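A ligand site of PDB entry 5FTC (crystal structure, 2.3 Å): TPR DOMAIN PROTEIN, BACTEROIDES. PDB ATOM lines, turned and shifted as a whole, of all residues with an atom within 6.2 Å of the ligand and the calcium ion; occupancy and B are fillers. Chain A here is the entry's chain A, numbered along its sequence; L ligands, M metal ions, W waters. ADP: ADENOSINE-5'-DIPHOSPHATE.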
ATOM      1  N   MET A   1       3.545  29.255  17.361  1.00  0.00           N
ATOM      2  CA  MET A   1       2.198  29.026  17.889  1.00  0.00           C
ATOM      3  C   MET A   1       2.237  28.780  19.386  1.00  0.00           C
ATOM      4  O   MET A   1       3.083  28.027  19.887  1.00  0.00           O
ATOM      5  CB  MET A   1       1.516  27.850  17.191  1.00  0.00           C
ATOM      6  CG  MET A   1       0.048  27.657  17.613  1.00  0.00           C
ATOM      7  SD  MET A   1      -0.865  26.324  16.754  1.00  0.00           S
ATOM      8  CE  MET A   1      -2.495  26.557  17.464  1.00  0.00           C
ATOM      9  N   ASP A   3      -1.052  28.734  21.473  1.00  0.00           N
ATOM     10  CA  ASP A   3      -2.250  28.121  22.013  1.00  0.00           C
ATOM     11  C   ASP A   3      -2.481  26.731  21.406  1.00  0.00           C
ATOM     12  O   ASP A   3      -3.611  26.258  21.305  1.00  0.00           O
ATOM     13  CB  ASP A   3      -3.469  29.027  21.801  1.00  0.00           C
ATOM     14  CG  ASP A   3      -3.722  29.362  20.332  1.00  0.00           C
ATOM     15  OD1 ASP A   3      -2.907  28.980  19.467  1.00  0.00           O
ATOM     16  OD2 ASP A   3      -4.745  30.029  20.053  1.00  0.00           O
ATOM     17  N   MET A   4      -1.392  26.073  21.021  1.00  0.00           N
ATOM     18  CA  MET A   4      -1.472  24.732  20.450  1.00  0.00           C
ATOM     19  C   MET A   4      -2.020  23.712  21.455  1.00  0.00           C
ATOM     20  O   MET A   4      -1.713  23.753  22.653  1.00  0.00           O
ATOM     21  CB  MET A   4      -0.099  24.287  19.954  1.00  0.00           C
ATOM     22  CG  MET A   4      -0.060  22.821  19.537  1.00  0.00           C
ATOM     23  SD  MET A   4       1.617  22.190  19.293  1.00  0.00           S
ATOM     24  CE  MET A   4       1.326  20.487  18.771  1.00  0.00           C
ATOM     25  N   ILE A   5      -2.834  22.796  20.950  1.00  0.00           N
ATOM     26  CA  ILE A   5      -3.447  21.754  21.766  1.00  0.00           C
ATOM     27  C   ILE A   5      -2.637  20.486  21.613  1.00  0.00           C
ATOM     28  O   ILE A   5      -2.309  20.083  20.493  1.00  0.00           O
ATOM     29  CB  ILE A   5      -4.924  21.529  21.364  1.00  0.00           C
ATOM     30  CG1 ILE A   5      -5.673  22.856  21.353  1.00  0.00           C
ATOM     31  CG2 ILE A   5      -5.606  20.528  22.302  1.00  0.00           C
ATOM     32  CD1 ILE A   5      -5.884  23.430  22.723  1.00  0.00           C
ATOM     33  N   LEU A   6      -2.294  19.848  22.721  1.00  0.00           N
ATOM     34  CA  LEU A   6      -1.584  18.572  22.672  1.00  0.00           C
ATOM     35  C   LEU A   6      -2.625  17.471  22.864  1.00  0.00           C
ATOM     36  O   LEU A   6      -3.201  17.330  23.949  1.00  0.00           O
ATOM     37  CB  LEU A   6      -0.489  18.503  23.738  1.00  0.00           C
ATOM     38  CG  LEU A   6       0.478  17.303  23.633  1.00  0.00           C
ATOM     39  CD1 LEU A   6       1.257  17.349  22.337  1.00  0.00           C
ATOM     40  CD2 LEU A   6       1.421  17.312  24.823  1.00  0.00           C
ATOM     41  N   THR A   7      -2.880  16.727  21.805  1.00  0.00           N
ATOM     42  CA  THR A   7      -3.851  15.654  21.828  1.00  0.00           C
ATOM     43  C   THR A   7      -3.196  14.351  22.249  1.00  0.00           C
ATOM     44  O   THR A   7      -1.975  14.186  22.170  1.00  0.00           O
ATOM     45  CB  THR A   7      -4.502  15.484  20.461  1.00  0.00           C
ATOM     46  OG1 THR A   7      -3.535  14.936  19.552  1.00  0.00           O
ATOM     47  CG2 THR A   7      -5.002  16.820  19.931  1.00  0.00           C
ATOM     48  N   MET A  10      -1.140  12.896  19.461  1.00  0.00           N
ATOM     49  CA  MET A  10       0.178  13.523  19.288  1.00  0.00           C
ATOM     50  C   MET A  10       1.139  13.023  20.348  1.00  0.00           C
ATOM     51  O   MET A  10       2.298  12.704  20.048  1.00  0.00           O
ATOM     52  CB  MET A  10       0.061  15.050  19.326  1.00  0.00           C
ATOM     53  CG  MET A  10      -0.731  15.641  18.126  1.00  0.00           C
ATOM     54  SD  MET A  10      -1.235  17.377  18.286  1.00  0.00           S
ATOM     55  CE  MET A  10      -0.872  17.644  19.993  1.00  0.00           C
ATOM     56  N   GLY A  28      -3.189  11.462   8.527  1.00  0.00           N
ATOM     57  CA  GLY A  28      -4.423  12.170   8.850  1.00  0.00           C
ATOM     58  C   GLY A  28      -4.804  13.112   7.731  1.00  0.00           C
ATOM     59  O   GLY A  28      -4.010  13.474   6.862  1.00  0.00           O
ATOM     60  N   LYS A  29      -6.068  13.518   7.737  1.00  0.00           N
ATOM     61  CA  LYS A  29      -6.588  14.332   6.655  1.00  0.00           C
ATOM     62  C   LYS A  29      -6.078  15.770   6.760  1.00  0.00           C
ATOM     63  O   LYS A  29      -5.492  16.183   7.772  1.00  0.00           O
ATOM     64  CB  LYS A  29      -8.128  14.310   6.672  1.00  0.00           C
ATOM     65  CG  LYS A  29      -8.724  12.932   6.365  1.00  0.00           C
ATOM     66  CD  LYS A  29     -10.239  12.994   6.290  1.00  0.00           C
ATOM     67  CE  LYS A  29     -10.868  11.605   6.395  1.00  0.00           C
ATOM     68  NZ  LYS A  29     -10.735  11.045   7.765  1.00  0.00           N
ATOM     69  N   ALA A  30      -6.298  16.520   5.686  1.00  0.00           N
ATOM     70  CA  ALA A  30      -6.068  17.958   5.709  1.00  0.00           C
ATOM     71  C   ALA A  30      -6.786  18.566   6.897  1.00  0.00           C
ATOM     72  O   ALA A  30      -7.955  18.252   7.163  1.00  0.00           O
ATOM     73  CB  ALA A  30      -6.555  18.579   4.396  1.00  0.00           C
ATOM     74  N   GLY A  31      -6.081  19.410   7.646  1.00  0.00           N
ATOM     75  CA  GLY A  31      -6.648  20.075   8.806  1.00  0.00           C
ATOM     76  C   GLY A  31      -6.507  19.301  10.109  1.00  0.00           C
ATOM     77  O   GLY A  31      -7.010  19.775  11.135  1.00  0.00           O
ATOM     78  N   SER A  32      -5.841  18.152  10.122  1.00  0.00           N
ATOM     79  CA  SER A  32      -5.707  17.396  11.358  1.00  0.00           C
ATOM     80  C   SER A  32      -4.417  17.720  12.114  1.00  0.00           C
ATOM     81  O   SER A  32      -4.096  17.029  13.090  1.00  0.00           O
ATOM     82  CB  SER A  32      -5.781  15.885  11.075  1.00  0.00           C
ATOM     83  OG  SER A  32      -4.670  15.481  10.300  1.00  0.00           O
ATOM     84  N   GLY A  33      -3.668  18.735  11.672  1.00  0.00           N
ATOM     85  CA  GLY A  33      -2.546  19.244  12.434  1.00  0.00           C
ATOM     86  C   GLY A  33      -1.200  18.629  12.141  1.00  0.00           C
ATOM     87  O   GLY A  33      -0.309  18.689  12.993  1.00  0.00           O
ATOM     88  N   LYS A  34      -1.014  18.035  10.965  1.00  0.00           N
ATOM     89  CA  LYS A  34       0.281  17.414  10.666  1.00  0.00           C
ATOM     90  C   LYS A  34       1.395  18.453  10.588  1.00  0.00           C
ATOM     91  O   LYS A  34       2.455  18.289  11.205  1.00  0.00           O
ATOM     92  CB  LYS A  34       0.190  16.617   9.359  1.00  0.00           C
ATOM     93  CG  LYS A  34      -0.821  15.476   9.363  1.00  0.00           C
ATOM     94  CD  LYS A  34      -0.765  14.686   8.030  1.00  0.00           C
ATOM     95  CE  LYS A  34      -1.227  15.540   6.816  1.00  0.00           C
ATOM     96  NZ  LYS A  34      -2.608  16.224   6.976  1.00  0.00           N
ATOM     97  N   THR A  35       1.173  19.527   9.840  1.00  0.00           N
ATOM     98  CA  THR A  35       2.218  20.539   9.708  1.00  0.00           C
ATOM     99  C   THR A  35       2.554  21.196  11.043  1.00  0.00           C
ATOM    100  O   THR A  35       3.728  21.393  11.368  1.00  0.00           O
ATOM    101  CB  THR A  35       1.802  21.568   8.677  1.00  0.00           C
ATOM    102  OG1 THR A  35       2.158  21.066   7.393  1.00  0.00           O
ATOM    103  CG2 THR A  35       2.467  22.969   8.942  1.00  0.00           C
ATOM    104  N   THR A  36       1.535  21.523  11.844  1.00  0.00           N
ATOM    105  CA  THR A  36       1.806  22.124  13.140  1.00  0.00           C
ATOM    106  C   THR A  36       2.527  21.136  14.058  1.00  0.00           C
ATOM    107  O   THR A  36       3.510  21.501  14.699  1.00  0.00           O
ATOM    108  CB  THR A  36       0.499  22.610  13.792  1.00  0.00           C
ATOM    109  OG1 THR A  36      -0.212  23.456  12.876  1.00  0.00           O
ATOM    110  CG2 THR A  36       0.793  23.379  15.085  1.00  0.00           C
ATOM    111  N   PHE A  37       2.063  19.871  14.105  1.00  0.00           N
ATOM    112  CA  PHE A  37       2.701  18.909  14.994  1.00  0.00           C
ATOM    113  C   PHE A  37       4.134  18.613  14.572  1.00  0.00           C
ATOM    114  O   PHE A  37       4.989  18.395  15.441  1.00  0.00           O
ATOM    115  CB  PHE A  37       1.906  17.592  15.071  1.00  0.00           C
ATOM    116  CG  PHE A  37       2.565  16.537  15.941  1.00  0.00           C
ATOM    117  CD1 PHE A  37       2.665  16.723  17.314  1.00  0.00           C
ATOM    118  CD2 PHE A  37       3.093  15.387  15.391  1.00  0.00           C
ATOM    119  CE1 PHE A  37       3.258  15.752  18.115  1.00  0.00           C
ATOM    120  CE2 PHE A  37       3.680  14.416  16.180  1.00  0.00           C
ATOM    121  CZ  PHE A  37       3.770  14.602  17.549  1.00  0.00           C
ATOM    122  N   ASP A 105       8.479  14.961   4.920  1.00  0.00           N
ATOM    123  CA  ASP A 105       7.136  15.480   4.808  1.00  0.00           C
ATOM    124  C   ASP A 105       6.521  15.127   3.455  1.00  0.00           C
ATOM    125  O   ASP A 105       7.235  14.938   2.459  1.00  0.00           O
ATOM    126  CB  ASP A 105       7.123  16.986   5.030  1.00  0.00           C
ATOM    127  CG  ASP A 105       5.765  17.500   5.526  1.00  0.00           C
ATOM    128  OD1 ASP A 105       5.021  16.702   6.124  1.00  0.00           O
ATOM    129  OD2 ASP A 105       5.471  18.692   5.328  1.00  0.00           O
ATOM    130  N   GLU A 106       5.193  15.035   3.420  1.00  0.00           N
ATOM    131  CA  GLU A 106       4.465  14.587   2.226  1.00  0.00           C
ATOM    132  C   GLU A 106       5.002  13.239   1.766  1.00  0.00           C
ATOM    133  O   GLU A 106       5.283  13.028   0.575  1.00  0.00           O
ATOM    134  CB  GLU A 106       4.527  15.601   1.091  1.00  0.00           C
ATOM    135  CG  GLU A 106       4.034  16.981   1.426  1.00  0.00           C
ATOM    136  CD  GLU A 106       2.525  17.042   1.585  1.00  0.00           C
ATOM    137  OE1 GLU A 106       1.815  16.931   0.565  1.00  0.00           O
ATOM    138  OE2 GLU A 106       2.065  17.196   2.731  1.00  0.00           O
ATOM    139  N   PHE A 187      -9.149  20.479  13.544  1.00  0.00           N
ATOM    140  CA  PHE A 187      -9.258  21.647  14.422  1.00  0.00           C
ATOM    141  C   PHE A 187     -10.202  22.718  13.868  1.00  0.00           C
ATOM    142  O   PHE A 187     -10.956  23.333  14.632  1.00  0.00           O
ATOM    143  CB  PHE A 187      -7.869  22.225  14.688  1.00  0.00           C
ATOM    144  CG  PHE A 187      -7.001  21.322  15.533  1.00  0.00           C
ATOM    145  CD1 PHE A 187      -7.184  21.231  16.904  1.00  0.00           C
ATOM    146  CD2 PHE A 187      -6.024  20.526  14.950  1.00  0.00           C
ATOM    147  CE1 PHE A 187      -6.406  20.383  17.684  1.00  0.00           C
ATOM    148  CE2 PHE A 187      -5.238  19.668  15.734  1.00  0.00           C
ATOM    149  CZ  PHE A 187      -5.429  19.596  17.101  1.00  0.00           C
ATOM    150  N   ARG A 188     -10.198  22.947  12.555  1.00  0.00           N
ATOM    151  CA  ARG A 188     -11.019  24.007  11.979  1.00  0.00           C
ATOM    152  C   ARG A 188     -12.508  23.811  12.278  1.00  0.00           C
ATOM    153  O   ARG A 188     -13.219  24.776  12.579  1.00  0.00           O
ATOM    154  CB  ARG A 188     -10.780  24.079  10.469  1.00  0.00           C
ATOM    155  CG  ARG A 188     -11.544  25.168   9.731  1.00  0.00           C
ATOM    156  CD  ARG A 188     -10.657  26.358   9.450  1.00  0.00           C
ATOM    157  NE  ARG A 188      -9.401  25.949   8.839  1.00  0.00           N
ATOM    158  CZ  ARG A 188      -8.365  26.770   8.664  1.00  0.00           C
ATOM    159  NH1 ARG A 188      -8.470  28.039   9.051  1.00  0.00           N
ATOM    160  NH2 ARG A 188      -7.245  26.324   8.106  1.00  0.00           N
ATOM    161  N   ASN A 288       0.396  31.829   6.161  1.00  0.00           N
ATOM    162  CA  ASN A 288      -0.308  31.967   7.428  1.00  0.00           C
ATOM    163  C   ASN A 288       0.283  33.115   8.234  1.00  0.00           C
ATOM    164  O   ASN A 288       1.502  33.278   8.323  1.00  0.00           O
ATOM    165  CB  ASN A 288      -0.232  30.688   8.257  1.00  0.00           C
ATOM    166  CG  ASN A 288      -0.945  29.526   7.590  1.00  0.00           C
ATOM    167  OD1 ASN A 288      -2.104  29.626   7.188  1.00  0.00           O
ATOM    168  ND2 ASN A 288      -0.238  28.408   7.457  1.00  0.00           N
ATOM    169  N   TYR A 295      -4.734  33.021   6.751  1.00  0.00           N
ATOM    170  CA  TYR A 295      -4.129  31.703   6.692  1.00  0.00           C
ATOM    171  C   TYR A 295      -3.974  31.292   5.240  1.00  0.00           C
ATOM    172  O   TYR A 295      -4.583  31.880   4.343  1.00  0.00           O
ATOM    173  CB  TYR A 295      -4.945  30.646   7.452  1.00  0.00           C
ATOM    174  CG  TYR A 295      -6.394  30.497   6.980  1.00  0.00           C
ATOM    175  CD1 TYR A 295      -6.691  29.734   5.855  1.00  0.00           C
ATOM    176  CD2 TYR A 295      -7.438  31.092   7.659  1.00  0.00           C
ATOM    177  CE1 TYR A 295      -7.995  29.574   5.421  1.00  0.00           C
ATOM    178  CE2 TYR A 295      -8.740  30.952   7.225  1.00  0.00           C
ATOM    179  CZ  TYR A 295      -9.019  30.188   6.106  1.00  0.00           C
ATOM    180  OH  TYR A 295     -10.318  30.038   5.663  1.00  0.00           O
ATOM    181  N   GLY A 365      -3.912  19.733   0.499  1.00  0.00           N
ATOM    182  CA  GLY A 365      -3.777  20.257   1.840  1.00  0.00           C
ATOM    183  C   GLY A 365      -4.694  21.421   2.196  1.00  0.00           C
ATOM    184  O   GLY A 365      -4.596  21.919   3.325  1.00  0.00           O
HETATM  185  PB  ADP L   1      -2.582  19.727   8.282  1.00  0.00           P
HETATM  186  O1B ADP L   1      -2.928  18.329   8.767  1.00  0.00           O
HETATM  187  O2B ADP L   1      -1.159  19.925   7.897  1.00  0.00           O
HETATM  188  O3B ADP L   1      -3.518  20.255   7.217  1.00  0.00           O
HETATM  189  PA  ADP L   1      -2.341  22.123   9.976  1.00  0.00           P
HETATM  190  O1A ADP L   1      -2.077  22.844   8.685  1.00  0.00           O
HETATM  191  O2A ADP L   1      -1.262  22.014  11.018  1.00  0.00           O
HETATM  192  O3A ADP L   1      -2.847  20.605   9.624  1.00  0.00           O
HETATM  193  O5' ADP L   1      -3.670  22.762  10.631  1.00  0.00           O
HETATM  194  C5' ADP L   1      -4.127  24.047  10.182  1.00  0.00           C
HETATM  195  C4' ADP L   1      -5.260  24.577  11.048  1.00  0.00           C
HETATM  196  O4' ADP L   1      -5.474  23.726  12.195  1.00  0.00           O
HETATM  197  C3' ADP L   1      -4.947  25.967  11.566  1.00  0.00           C
HETATM  198  O3' ADP L   1      -6.149  26.734  11.685  1.00  0.00           O
HETATM  199  C2' ADP L   1      -4.309  25.676  12.906  1.00  0.00           C
HETATM  200  O2' ADP L   1      -4.456  26.768  13.819  1.00  0.00           O
HETATM  201  C1' ADP L   1      -5.082  24.443  13.376  1.00  0.00           C
HETATM  202  N9  ADP L   1      -4.270  23.587  14.273  1.00  0.00           N
HETATM  203  C8  ADP L   1      -3.361  22.672  13.866  1.00  0.00           C
HETATM  204  N7  ADP L   1      -2.801  22.045  14.928  1.00  0.00           N
HETATM  205  C5  ADP L   1      -3.348  22.565  16.032  1.00  0.00           C
HETATM  206  C6  ADP L   1      -3.197  22.338  17.480  1.00  0.00           C
HETATM  207  N6  ADP L   1      -2.320  21.419  17.918  1.00  0.00           N
HETATM  208  N1  ADP L   1      -3.947  23.086  18.321  1.00  0.00           N
HETATM  209  C2  ADP L   1      -4.831  24.006  17.871  1.00  0.00           C
HETATM  210  N3  ADP L   1      -5.016  24.251  16.557  1.00  0.00           N
HETATM  211  C4  ADP L   1      -4.330  23.574  15.606  1.00  0.00           C
HETATM  212 CA    CA M   1       0.096  20.516   5.899  1.00  0.00          CA
HETATM  213  O   HOH W   1      -0.070  19.011   4.043  1.00  0.00           O
HETATM  214  O   HOH W   2       1.426  18.186   5.895  1.00  0.00           O
HETATM  215  O   HOH W   3      -0.840  22.681   6.362  1.00  0.00           O
HETATM  216  O   HOH W   4       1.216  21.558   4.111  1.00  0.00           O
HETATM  217  O   HOH W   5      -0.963  19.982  15.636  1.00  0.00           O
HETATM  218  O   HOH W   6      -2.357  20.135   5.066  1.00  0.00           O
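OG of Ser 32 lies within hydrogen-bond range of O of Lys 29 (2.7 Å).
The backbone NH (N) of Phe 187 is in hydrogen-bond range of the backbone carbonyl oxygen (O) of Gly 31 (3.3 Å).
The backbone carbonyl oxygen (O) of Gly 28 lies within hydrogen-bond range of the side-chain amino group (NZ) of Lys 34.
O of Lys 29 lies within hydrogen-bond range of NZ of Lys 34.
O1B of the ligand sits close to O of Lys 29.
Met 1 touches the ligand.
Met 4 touches the ligand (CG to N6, 3.1 Å).
C of Ala 30 touches O3B of the ligand (3.7 Å).
Phe 187 touches the ligand (CE2 to C5, 3.5 Å).
NH1 of Arg 188 touches O3' of the ligand, at 3.7 Å.
13 residues have an atom within 4 Å of the ligand: Met 1, Met 4, Ile 5, Lys 29, Ala 30, Gly 31, Ser 32, Gly 33, Lys 34, Thr 35, Thr 36, Phe 187 and Arg 188.
The nearest printed residue that does not touch the ligand is Met 10 (4.2 Å).
Water W6 bridges an oxygen (O3B) of the ligand and the backbone carbonyl oxygen of Gly 365.
NZ of Lys 34 lies within salt-bridge range of O1B of the ligand, at 2.8 Å.
An oxygen (O1B) of the ligand lies within hydrogen-bond range of the backbone NH (N) of Ser 32, at 3.2 Å.
O of Ile 5 lies within hydrogen-bond range of N6 of the ligand (2.9 Å).
The backbone NH (N) of Lys 34 lies within hydrogen-bond range of an oxygen (O1B) of the ligand (2.9 Å).
The backbone NH (N) of Thr 35 lies close to an oxygen (O2B) of the ligand.
The side-chain hydroxyl (OG1) of Thr 36 lies within hydrogen-bond range of an oxygen (O2A) of the ligand, at 2.6 Å.
N of Thr 36 lies within hydrogen-bond range of O2A of the ligand.
The backbone NH (N) of Ile 5 sits at hydrogen-bond distance from a nitrogen (N1) of the ligand, at 2.9 Å.
An oxygen (O3B) of the ligand is in hydrogen-bond range of the backbone NH (N) of Gly 31, at 2.7 Å.
The backbone NH of Gly 33 lies within hydrogen-bond range of an oxygen (O3A) of the ligand (2.9 Å).
Within 4 Å of the calcium ion: Thr 35.
The calcium ion is bound by water W4 (2.4 Å), water W1 (2.4 Å), water W3 (2.4 Å), O2B of the ligand (2.4 Å), OG1 of Thr 35 (2.6 Å), water W6 (2.6 Å) and water W2 (2.7 Å).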
